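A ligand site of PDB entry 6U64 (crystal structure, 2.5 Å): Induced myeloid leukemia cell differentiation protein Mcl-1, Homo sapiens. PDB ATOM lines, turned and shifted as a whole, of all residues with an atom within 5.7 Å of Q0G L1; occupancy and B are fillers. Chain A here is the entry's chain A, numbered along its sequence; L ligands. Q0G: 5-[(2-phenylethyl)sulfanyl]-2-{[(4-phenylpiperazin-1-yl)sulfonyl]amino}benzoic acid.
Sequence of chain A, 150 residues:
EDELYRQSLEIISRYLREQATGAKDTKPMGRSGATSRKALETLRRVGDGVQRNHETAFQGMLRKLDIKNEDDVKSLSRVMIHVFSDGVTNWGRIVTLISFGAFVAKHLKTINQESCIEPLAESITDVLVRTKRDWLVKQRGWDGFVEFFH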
ATOM      1  N   PHE A  58     -13.310  -5.278  -3.942  1.00  0.00           N
ATOM      2  CA  PHE A  58     -12.878  -3.870  -3.854  1.00  0.00           C
ATOM      3  C   PHE A  58     -11.318  -3.734  -3.900  1.00  0.00           C
ATOM      4  O   PHE A  58     -10.802  -2.907  -4.662  1.00  0.00           O
ATOM      5  CB  PHE A  58     -13.487  -3.203  -2.613  1.00  0.00           C
ATOM      6  CG  PHE A  58     -14.934  -2.774  -2.791  1.00  0.00           C
ATOM      7  CD1 PHE A  58     -15.630  -3.053  -3.964  1.00  0.00           C
ATOM      8  CD2 PHE A  58     -15.592  -2.043  -1.800  1.00  0.00           C
ATOM      9  CE1 PHE A  58     -16.942  -2.617  -4.155  1.00  0.00           C
ATOM     10  CE2 PHE A  58     -16.902  -1.594  -1.997  1.00  0.00           C
ATOM     11  CZ  PHE A  58     -17.567  -1.892  -3.171  1.00  0.00           C
ATOM     12  N   MET A  61     -10.223  -4.663  -7.638  1.00  0.00           N
ATOM     13  CA  MET A  61     -10.503  -3.576  -8.582  1.00  0.00           C
ATOM     14  C   MET A  61      -9.527  -2.417  -8.392  1.00  0.00           C
ATOM     15  O   MET A  61      -9.053  -1.858  -9.373  1.00  0.00           O
ATOM     16  CB  MET A  61     -11.954  -3.085  -8.458  1.00  0.00           C
ATOM     17  CG  MET A  61     -13.001  -4.117  -8.935  1.00  0.00           C
ATOM     18  SD  MET A  61     -14.681  -3.440  -9.077  1.00  0.00           S
ATOM     19  CE  MET A  61     -15.148  -3.340  -7.335  1.00  0.00           C
ATOM     20  N   LYS A  64      -6.031  -3.342  -9.628  1.00  0.00           N
ATOM     21  CA  LYS A  64      -6.103  -3.327 -11.080  1.00  0.00           C
ATOM     22  C   LYS A  64      -6.209  -1.906 -11.635  1.00  0.00           C
ATOM     23  O   LYS A  64      -5.450  -1.590 -12.536  1.00  0.00           O
ATOM     24  CB  LYS A  64      -7.244  -4.195 -11.623  1.00  0.00           C
ATOM     25  CG  LYS A  64      -6.955  -5.687 -11.546  1.00  0.00           C
ATOM     26  CD  LYS A  64      -8.246  -6.517 -11.724  1.00  0.00           C
ATOM     27  CE  LYS A  64      -8.133  -7.989 -11.331  1.00  0.00           C
ATOM     28  NZ  LYS A  64      -6.932  -8.668 -11.895  1.00  0.00           N
ATOM     29  N   LEU A  65      -7.071  -1.042 -11.075  1.00  0.00           N
ATOM     30  CA  LEU A  65      -7.221   0.325 -11.603  1.00  0.00           C
ATOM     31  C   LEU A  65      -6.043   1.268 -11.206  1.00  0.00           C
ATOM     32  O   LEU A  65      -5.867   2.281 -11.881  1.00  0.00           O
ATOM     33  CB  LEU A  65      -8.549   0.962 -11.207  1.00  0.00           C
ATOM     34  CG  LEU A  65      -9.817   0.278 -11.698  1.00  0.00           C
ATOM     35  CD1 LEU A  65     -11.042   0.897 -11.061  1.00  0.00           C
ATOM     36  CD2 LEU A  65      -9.917   0.307 -13.216  1.00  0.00           C
ATOM     37  N   LEU A  76     -10.597   7.228 -15.328  1.00  0.00           N
ATOM     38  CA  LEU A  76     -11.465   6.144 -14.855  1.00  0.00           C
ATOM     39  C   LEU A  76     -12.948   6.526 -15.027  1.00  0.00           C
ATOM     40  O   LEU A  76     -13.723   5.674 -15.475  1.00  0.00           O
ATOM     41  CB  LEU A  76     -11.177   5.743 -13.386  1.00  0.00           C
ATOM     42  N   VAL A  79     -14.413   5.925 -18.398  1.00  0.00           N
ATOM     43  CA  VAL A  79     -14.645   4.502 -18.674  1.00  0.00           C
ATOM     44  C   VAL A  79     -15.861   4.007 -17.837  1.00  0.00           C
ATOM     45  O   VAL A  79     -16.720   3.282 -18.366  1.00  0.00           O
ATOM     46  CB  VAL A  79     -13.373   3.652 -18.435  1.00  0.00           C
ATOM     47  CG1 VAL A  79     -13.637   2.176 -18.678  1.00  0.00           C
ATOM     48  CG2 VAL A  79     -12.249   4.140 -19.346  1.00  0.00           C
ATOM     49  N   MET A  80     -15.928   4.457 -16.568  1.00  0.00           N
ATOM     50  CA  MET A  80     -16.928   4.143 -15.562  1.00  0.00           C
ATOM     51  C   MET A  80     -18.329   4.612 -16.031  1.00  0.00           C
ATOM     52  O   MET A  80     -19.278   3.863 -15.824  1.00  0.00           O
ATOM     53  CB  MET A  80     -16.500   4.790 -14.234  1.00  0.00           C
ATOM     54  CG  MET A  80     -17.113   4.159 -12.988  1.00  0.00           C
ATOM     55  SD  MET A  80     -16.179   4.470 -11.443  1.00  0.00           S
ATOM     56  CE  MET A  80     -16.364   6.226 -11.261  1.00  0.00           C
ATOM     57  N   VAL A  83     -19.554   1.860 -18.714  1.00  0.00           N
ATOM     58  CA  VAL A  83     -19.854   0.533 -18.179  1.00  0.00           C
ATOM     59  C   VAL A  83     -20.992   0.598 -17.153  1.00  0.00           C
ATOM     60  O   VAL A  83     -21.760  -0.360 -17.068  1.00  0.00           O
ATOM     61  CB  VAL A  83     -18.634  -0.334 -17.673  1.00  0.00           C
ATOM     62  CG1 VAL A  83     -17.264   0.176 -18.119  1.00  0.00           C
ATOM     63  CG2 VAL A  83     -18.659  -0.663 -16.184  1.00  0.00           C
ATOM     64  N   PHE A  84     -21.162   1.730 -16.431  1.00  0.00           N
ATOM     65  CA  PHE A  84     -22.233   1.813 -15.442  1.00  0.00           C
ATOM     66  C   PHE A  84     -23.614   2.035 -16.100  1.00  0.00           C
ATOM     67  O   PHE A  84     -24.629   1.693 -15.488  1.00  0.00           O
ATOM     68  CB  PHE A  84     -21.944   2.911 -14.409  1.00  0.00           C
ATOM     69  CG  PHE A  84     -22.701   2.764 -13.110  1.00  0.00           C
ATOM     70  CD1 PHE A  84     -22.421   1.719 -12.232  1.00  0.00           C
ATOM     71  CD2 PHE A  84     -23.667   3.689 -12.741  1.00  0.00           C
ATOM     72  CE1 PHE A  84     -23.123   1.588 -11.035  1.00  0.00           C
ATOM     73  CE2 PHE A  84     -24.370   3.558 -11.544  1.00  0.00           C
ATOM     74  CZ  PHE A  84     -24.090   2.514 -10.701  1.00  0.00           C
ATOM     75  N   ASP A  86     -24.640   0.387 -18.663  1.00  0.00           N
ATOM     76  CA  ASP A  86     -25.033  -0.933 -19.150  1.00  0.00           C
ATOM     77  C   ASP A  86     -25.622  -1.786 -18.031  1.00  0.00           C
ATOM     78  O   ASP A  86     -25.156  -1.685 -16.894  1.00  0.00           O
ATOM     79  CB  ASP A  86     -23.825  -1.675 -19.776  1.00  0.00           C
ATOM     80  CG  ASP A  86     -24.271  -2.885 -20.569  1.00  0.00           C
ATOM     81  OD1 ASP A  86     -25.078  -2.700 -21.524  1.00  0.00           O
ATOM     82  OD2 ASP A  86     -23.911  -4.010 -20.174  1.00  0.00           O
ATOM     83  N   ARG A  93     -26.595  -1.768  -6.594  1.00  0.00           N
ATOM     84  CA  ARG A  93     -25.607  -1.413  -7.576  1.00  0.00           C
ATOM     85  C   ARG A  93     -25.160   0.035  -7.346  1.00  0.00           C
ATOM     86  O   ARG A  93     -23.984   0.357  -7.502  1.00  0.00           O
ATOM     87  CB  ARG A  93     -26.201  -1.584  -8.987  1.00  0.00           C
ATOM     88  CG  ARG A  93     -25.231  -1.197 -10.086  1.00  0.00           C
ATOM     89  CD  ARG A  93     -25.825  -1.197 -11.454  1.00  0.00           C
ATOM     90  NE  ARG A  93     -24.735  -1.214 -12.428  1.00  0.00           N
ATOM     91  CZ  ARG A  93     -24.875  -1.230 -13.743  1.00  0.00           C
ATOM     92  NH1 ARG A  93     -26.088  -1.205 -14.287  1.00  0.00           N
ATOM     93  NH2 ARG A  93     -23.807  -1.281 -14.523  1.00  0.00           N
ATOM     94  N   THR A  96     -23.046   0.170  -4.238  1.00  0.00           N
ATOM     95  CA  THR A  96     -21.738  -0.447  -4.475  1.00  0.00           C
ATOM     96  C   THR A  96     -20.826   0.579  -5.139  1.00  0.00           C
ATOM     97  O   THR A  96     -19.659   0.655  -4.789  1.00  0.00           O
ATOM     98  CB  THR A  96     -21.862  -1.739  -5.292  1.00  0.00           C
ATOM     99  OG1 THR A  96     -22.741  -2.612  -4.586  1.00  0.00           O
ATOM    100  CG2 THR A  96     -20.515  -2.436  -5.476  1.00  0.00           C
ATOM    101  N   LEU A  97     -21.367   1.375  -6.081  1.00  0.00           N
ATOM    102  CA  LEU A  97     -20.590   2.422  -6.719  1.00  0.00           C
ATOM    103  C   LEU A  97     -20.012   3.400  -5.659  1.00  0.00           C
ATOM    104  O   LEU A  97     -18.792   3.636  -5.639  1.00  0.00           O
ATOM    105  CB  LEU A  97     -21.432   3.179  -7.741  1.00  0.00           C
ATOM    106  CG  LEU A  97     -20.695   4.324  -8.393  1.00  0.00           C
ATOM    107  CD1 LEU A  97     -19.585   3.806  -9.314  1.00  0.00           C
ATOM    108  CD2 LEU A  97     -21.653   5.268  -9.089  1.00  0.00           C
ATOM    109  N   PHE A 100     -17.520   1.826  -3.293  1.00  0.00           N
ATOM    110  CA  PHE A 100     -16.225   1.703  -3.977  1.00  0.00           C
ATOM    111  C   PHE A 100     -15.518   3.047  -3.952  1.00  0.00           C
ATOM    112  O   PHE A 100     -14.321   3.066  -3.681  1.00  0.00           O
ATOM    113  CB  PHE A 100     -16.346   1.159  -5.404  1.00  0.00           C
ATOM    114  CG  PHE A 100     -15.005   0.948  -6.088  1.00  0.00           C
ATOM    115  CD1 PHE A 100     -14.062   0.074  -5.559  1.00  0.00           C
ATOM    116  CD2 PHE A 100     -14.688   1.649  -7.259  1.00  0.00           C
ATOM    117  CE1 PHE A 100     -12.817  -0.083  -6.167  1.00  0.00           C
ATOM    118  CE2 PHE A 100     -13.471   1.434  -7.901  1.00  0.00           C
ATOM    119  CZ  PHE A 100     -12.527   0.603  -7.344  1.00  0.00           C
HETATM  120  C25 Q0G L   1     -16.577   0.298  -9.791  1.00  0.00           C
HETATM  121  C24 Q0G L   1     -15.766  -0.189 -10.963  1.00  0.00           C
HETATM  122  C23 Q0G L   1     -14.170   1.297 -13.130  1.00  0.00           C
HETATM  123  N3  Q0G L   1     -16.224   0.439 -12.207  1.00  0.00           N
HETATM  124  C22 Q0G L   1     -13.252   1.353 -14.165  1.00  0.00           C
HETATM  125  O4  Q0G L   1     -20.228  -0.163  -8.743  1.00  0.00           O
HETATM  126  C20 Q0G L   1     -14.618  -0.095 -15.470  1.00  0.00           C
HETATM  127  C18 Q0G L   1     -15.327   0.531 -13.254  1.00  0.00           C
HETATM  128  C19 Q0G L   1     -15.540  -0.163 -14.444  1.00  0.00           C
HETATM  129  O3  Q0G L   1     -18.354  -1.629  -8.109  1.00  0.00           O
HETATM  130  C17 Q0G L   1     -17.650   0.183 -12.450  1.00  0.00           C
HETATM  131  C15 Q0G L   1     -19.147  -2.804 -11.155  1.00  0.00           C
HETATM  132  C16 Q0G L   1     -18.489   0.670 -11.266  1.00  0.00           C
HETATM  133  N2  Q0G L   1     -18.007   0.018 -10.037  1.00  0.00           N
HETATM  134  C21 Q0G L   1     -13.467   0.648 -15.327  1.00  0.00           C
HETATM  135  C14 Q0G L   1     -18.037  -3.547 -10.800  1.00  0.00           C
HETATM  136  C1  Q0G L   1     -20.932  -2.206 -12.840  1.00  0.00           C
HETATM  137  C13 Q0G L   1     -17.514  -4.468 -11.683  1.00  0.00           C
HETATM  138  C4  Q0G L   1     -18.067  -4.608 -12.937  1.00  0.00           C
HETATM  139  C5  Q0G L   1     -15.623  -4.353 -14.154  1.00  0.00           C
HETATM  140  O1  Q0G L   1     -21.224  -2.070 -14.018  1.00  0.00           O
HETATM  141  N1  Q0G L   1     -19.581  -1.761 -10.310  1.00  0.00           N
HETATM  142  C6  Q0G L   1     -14.542  -5.180 -13.502  1.00  0.00           C
HETATM  143  O2  Q0G L   1     -21.613  -1.693 -11.881  1.00  0.00           O
HETATM  144  C3  Q0G L   1     -19.220  -3.920 -13.287  1.00  0.00           C
HETATM  145  C2  Q0G L   1     -19.775  -3.011 -12.400  1.00  0.00           C
HETATM  146  C7  Q0G L   1     -13.255  -4.431 -13.337  1.00  0.00           C
HETATM  147  C12 Q0G L   1     -13.198  -3.257 -12.616  1.00  0.00           C
HETATM  148  C11 Q0G L   1     -11.999  -2.589 -12.442  1.00  0.00           C
HETATM  149  C10 Q0G L   1     -10.847  -3.064 -13.022  1.00  0.00           C
HETATM  150  C9  Q0G L   1     -10.894  -4.220 -13.771  1.00  0.00           C
HETATM  151  C8  Q0G L   1     -12.077  -4.917 -13.901  1.00  0.00           C
HETATM  152  S2  Q0G L   1     -19.052  -0.902  -9.101  1.00  0.00           S
HETATM  153  S1  Q0G L   1     -17.085  -5.408 -14.166  1.00  0.00           S
HETATM  154  C25 Q0G L   2     -18.057  -9.399  -8.100  1.00  0.00           C
HETATM  155  C24 Q0G L   2     -16.603  -9.044  -8.288  1.00  0.00           C
HETATM  156  C23 Q0G L   2     -15.109  -8.885 -11.600  1.00  0.00           C
HETATM  157  N3  Q0G L   2     -16.101  -9.646  -9.522  1.00  0.00           N
HETATM  158  C22 Q0G L   2     -14.059  -8.296 -12.294  1.00  0.00           C
HETATM  159  O4  Q0G L   2     -19.132 -13.021  -7.153  1.00  0.00           O
HETATM  160  C20 Q0G L   2     -12.906  -7.907 -10.227  1.00  0.00           C
HETATM  161  C18 Q0G L   2     -15.055  -9.010 -10.214  1.00  0.00           C
HETATM  162  C19 Q0G L   2     -13.951  -8.502  -9.528  1.00  0.00           C
HETATM  163  O3  Q0G L   2     -20.167 -10.908  -6.454  1.00  0.00           O
HETATM  164  C17 Q0G L   2     -16.186 -11.103  -9.436  1.00  0.00           C
HETATM  165  C15 Q0G L   2     -16.935 -12.149  -4.910  1.00  0.00           C
HETATM  166  C16 Q0G L   2     -17.634 -11.550  -9.227  1.00  0.00           C
HETATM  167  N2  Q0G L   2     -18.204 -10.866  -8.048  1.00  0.00           N
HETATM  168  C21 Q0G L   2     -12.965  -7.792 -11.599  1.00  0.00           C
HETATM  169  C14 Q0G L   2     -16.525 -13.394  -5.371  1.00  0.00           C
HETATM  170  C1  Q0G L   2     -16.639 -10.223  -3.285  1.00  0.00           C
HETATM  171  C13 Q0G L   2     -15.480 -14.059  -4.760  1.00  0.00           C
HETATM  172  C4  Q0G L   2     -14.860 -13.504  -3.660  1.00  0.00           C
HETATM  173  C5  Q0G L   2     -14.234 -16.055  -2.614  1.00  0.00           C
HETATM  174  O1  Q0G L   2     -15.890  -9.614  -2.553  1.00  0.00           O
HETATM  175  N1  Q0G L   2     -17.982 -11.455  -5.582  1.00  0.00           N
HETATM  176  C6  Q0G L   2     -15.329 -16.006  -1.562  1.00  0.00           C
HETATM  177  O2  Q0G L   2     -17.755  -9.714  -3.729  1.00  0.00           O
HETATM  178  C3  Q0G L   2     -15.270 -12.273  -3.158  1.00  0.00           C
HETATM  179  C2  Q0G L   2     -16.296 -11.572  -3.788  1.00  0.00           C
HETATM  180  C7  Q0G L   2     -15.790 -17.313  -0.953  1.00  0.00           C
HETATM  181  C12 Q0G L   2     -16.960 -17.357  -0.223  1.00  0.00           C
HETATM  182  C11 Q0G L   2     -17.307 -18.496   0.503  1.00  0.00           C
HETATM  183  C10 Q0G L   2     -16.508 -19.607   0.472  1.00  0.00           C
HETATM  184  C9  Q0G L   2     -15.357 -19.585  -0.280  1.00  0.00           C
HETATM  185  C8  Q0G L   2     -14.996 -18.448  -0.987  1.00  0.00           C
HETATM  186  S2  Q0G L   2     -19.004 -11.635  -6.859  1.00  0.00           S
HETATM  187  S1  Q0G L   2     -13.534 -14.408  -2.938  1.00  0.00           S
HETATM  188  C25 Q0G L   3     -25.296  -5.082 -13.632  1.00  0.00           C
HETATM  189  C24 Q0G L   3     -25.134  -5.413 -12.167  1.00  0.00           C
HETATM  190  C23 Q0G L   3     -22.624  -4.189  -9.671  1.00  0.00           C
HETATM  191  N3  Q0G L   3     -23.904  -4.862 -11.633  1.00  0.00           N
HETATM  192  C22 Q0G L   3     -22.539  -3.992  -8.295  1.00  0.00           C
HETATM  193  O4  Q0G L   3     -23.058  -6.999 -16.138  1.00  0.00           O
HETATM  194  C20 Q0G L   3     -24.730  -4.910  -8.005  1.00  0.00           C
HETATM  195  C18 Q0G L   3     -23.770  -4.740 -10.226  1.00  0.00           C
HETATM  196  C19 Q0G L   3     -24.818  -5.134  -9.371  1.00  0.00           C
HETATM  197  O3  Q0G L   3     -24.507  -5.095 -16.719  1.00  0.00           O
HETATM  198  C17 Q0G L   3     -22.799  -5.516 -12.343  1.00  0.00           C
HETATM  199  C15 Q0G L   3     -25.773  -8.341 -14.997  1.00  0.00           C
HETATM  200  C16 Q0G L   3     -22.827  -5.177 -13.800  1.00  0.00           C
HETATM  201  N2  Q0G L   3     -24.126  -5.575 -14.385  1.00  0.00           N
HETATM  202  C21 Q0G L   3     -23.601  -4.328  -7.471  1.00  0.00           C
HETATM  203  C14 Q0G L   3     -24.797  -8.908 -14.176  1.00  0.00           C
HETATM  204  C1  Q0G L   3     -28.200  -8.317 -15.827  1.00  0.00           C
HETATM  205  C13 Q0G L   3     -25.112  -9.950 -13.338  1.00  0.00           C
HETATM  206  C4  Q0G L   3     -26.393 -10.465 -13.320  1.00  0.00           C
HETATM  207  O1  Q0G L   3     -29.329  -8.786 -15.799  1.00  0.00           O
HETATM  208  N1  Q0G L   3     -25.478  -7.179 -15.733  1.00  0.00           N
HETATM  209  O2  Q0G L   3     -27.862  -7.311 -16.582  1.00  0.00           O
HETATM  210  C3  Q0G L   3     -27.382  -9.942 -14.139  1.00  0.00           C
HETATM  211  C2  Q0G L   3     -27.084  -8.882 -14.993  1.00  0.00           C
HETATM  212  S2  Q0G L   3     -24.184  -6.183 -15.862  1.00  0.00           S
HETATM  213  S1  Q0G L   3     -26.806 -11.834 -12.287  1.00  0.00           S
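An oxygen (O1) of Q0G L1 lies within salt-bridge range of the guanidinium group of Arg 93 (2.7 Å). An oxygen (O4) of Q0G L1 lies within hydrogen-bond range of the backbone NH (N) of Leu 97 (3.3 Å).
O of Phe 84 is in hydrogen-bond range of NH2 of Arg 93 (3.2 Å). O of Val 83 lies within hydrogen-bond range of NH2 of Arg 93. The guanidinium group (NH2) of Arg 93 lies within hydrogen-bond range of the backbone carbonyl oxygen (O) of Asp 86, 2.8 Å away.
Merely in contact with Q0G L1: Met 61 (3.7 Å), Leu 65 (3.5 Å), Val 79 (3.7 Å), Met 80 (3.9 Å), Val 83 (3.5 Å), Phe 84 (3.5 Å), Thr 96 (3.5 Å) and Phe 100 (3.4 Å). Hydrophobic or aromatic side chains within 4 Å of Q0G L1: Met 61, Leu 65, Val 79, Met 80, Val 83, Phe 84, Leu 97 and Phe 100. Of the 14 residues printed, 10 come within 4 Å of Q0G L1. The nearest printed residue that does not touch Q0G L1 is Lys 64 (4.03 Å).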
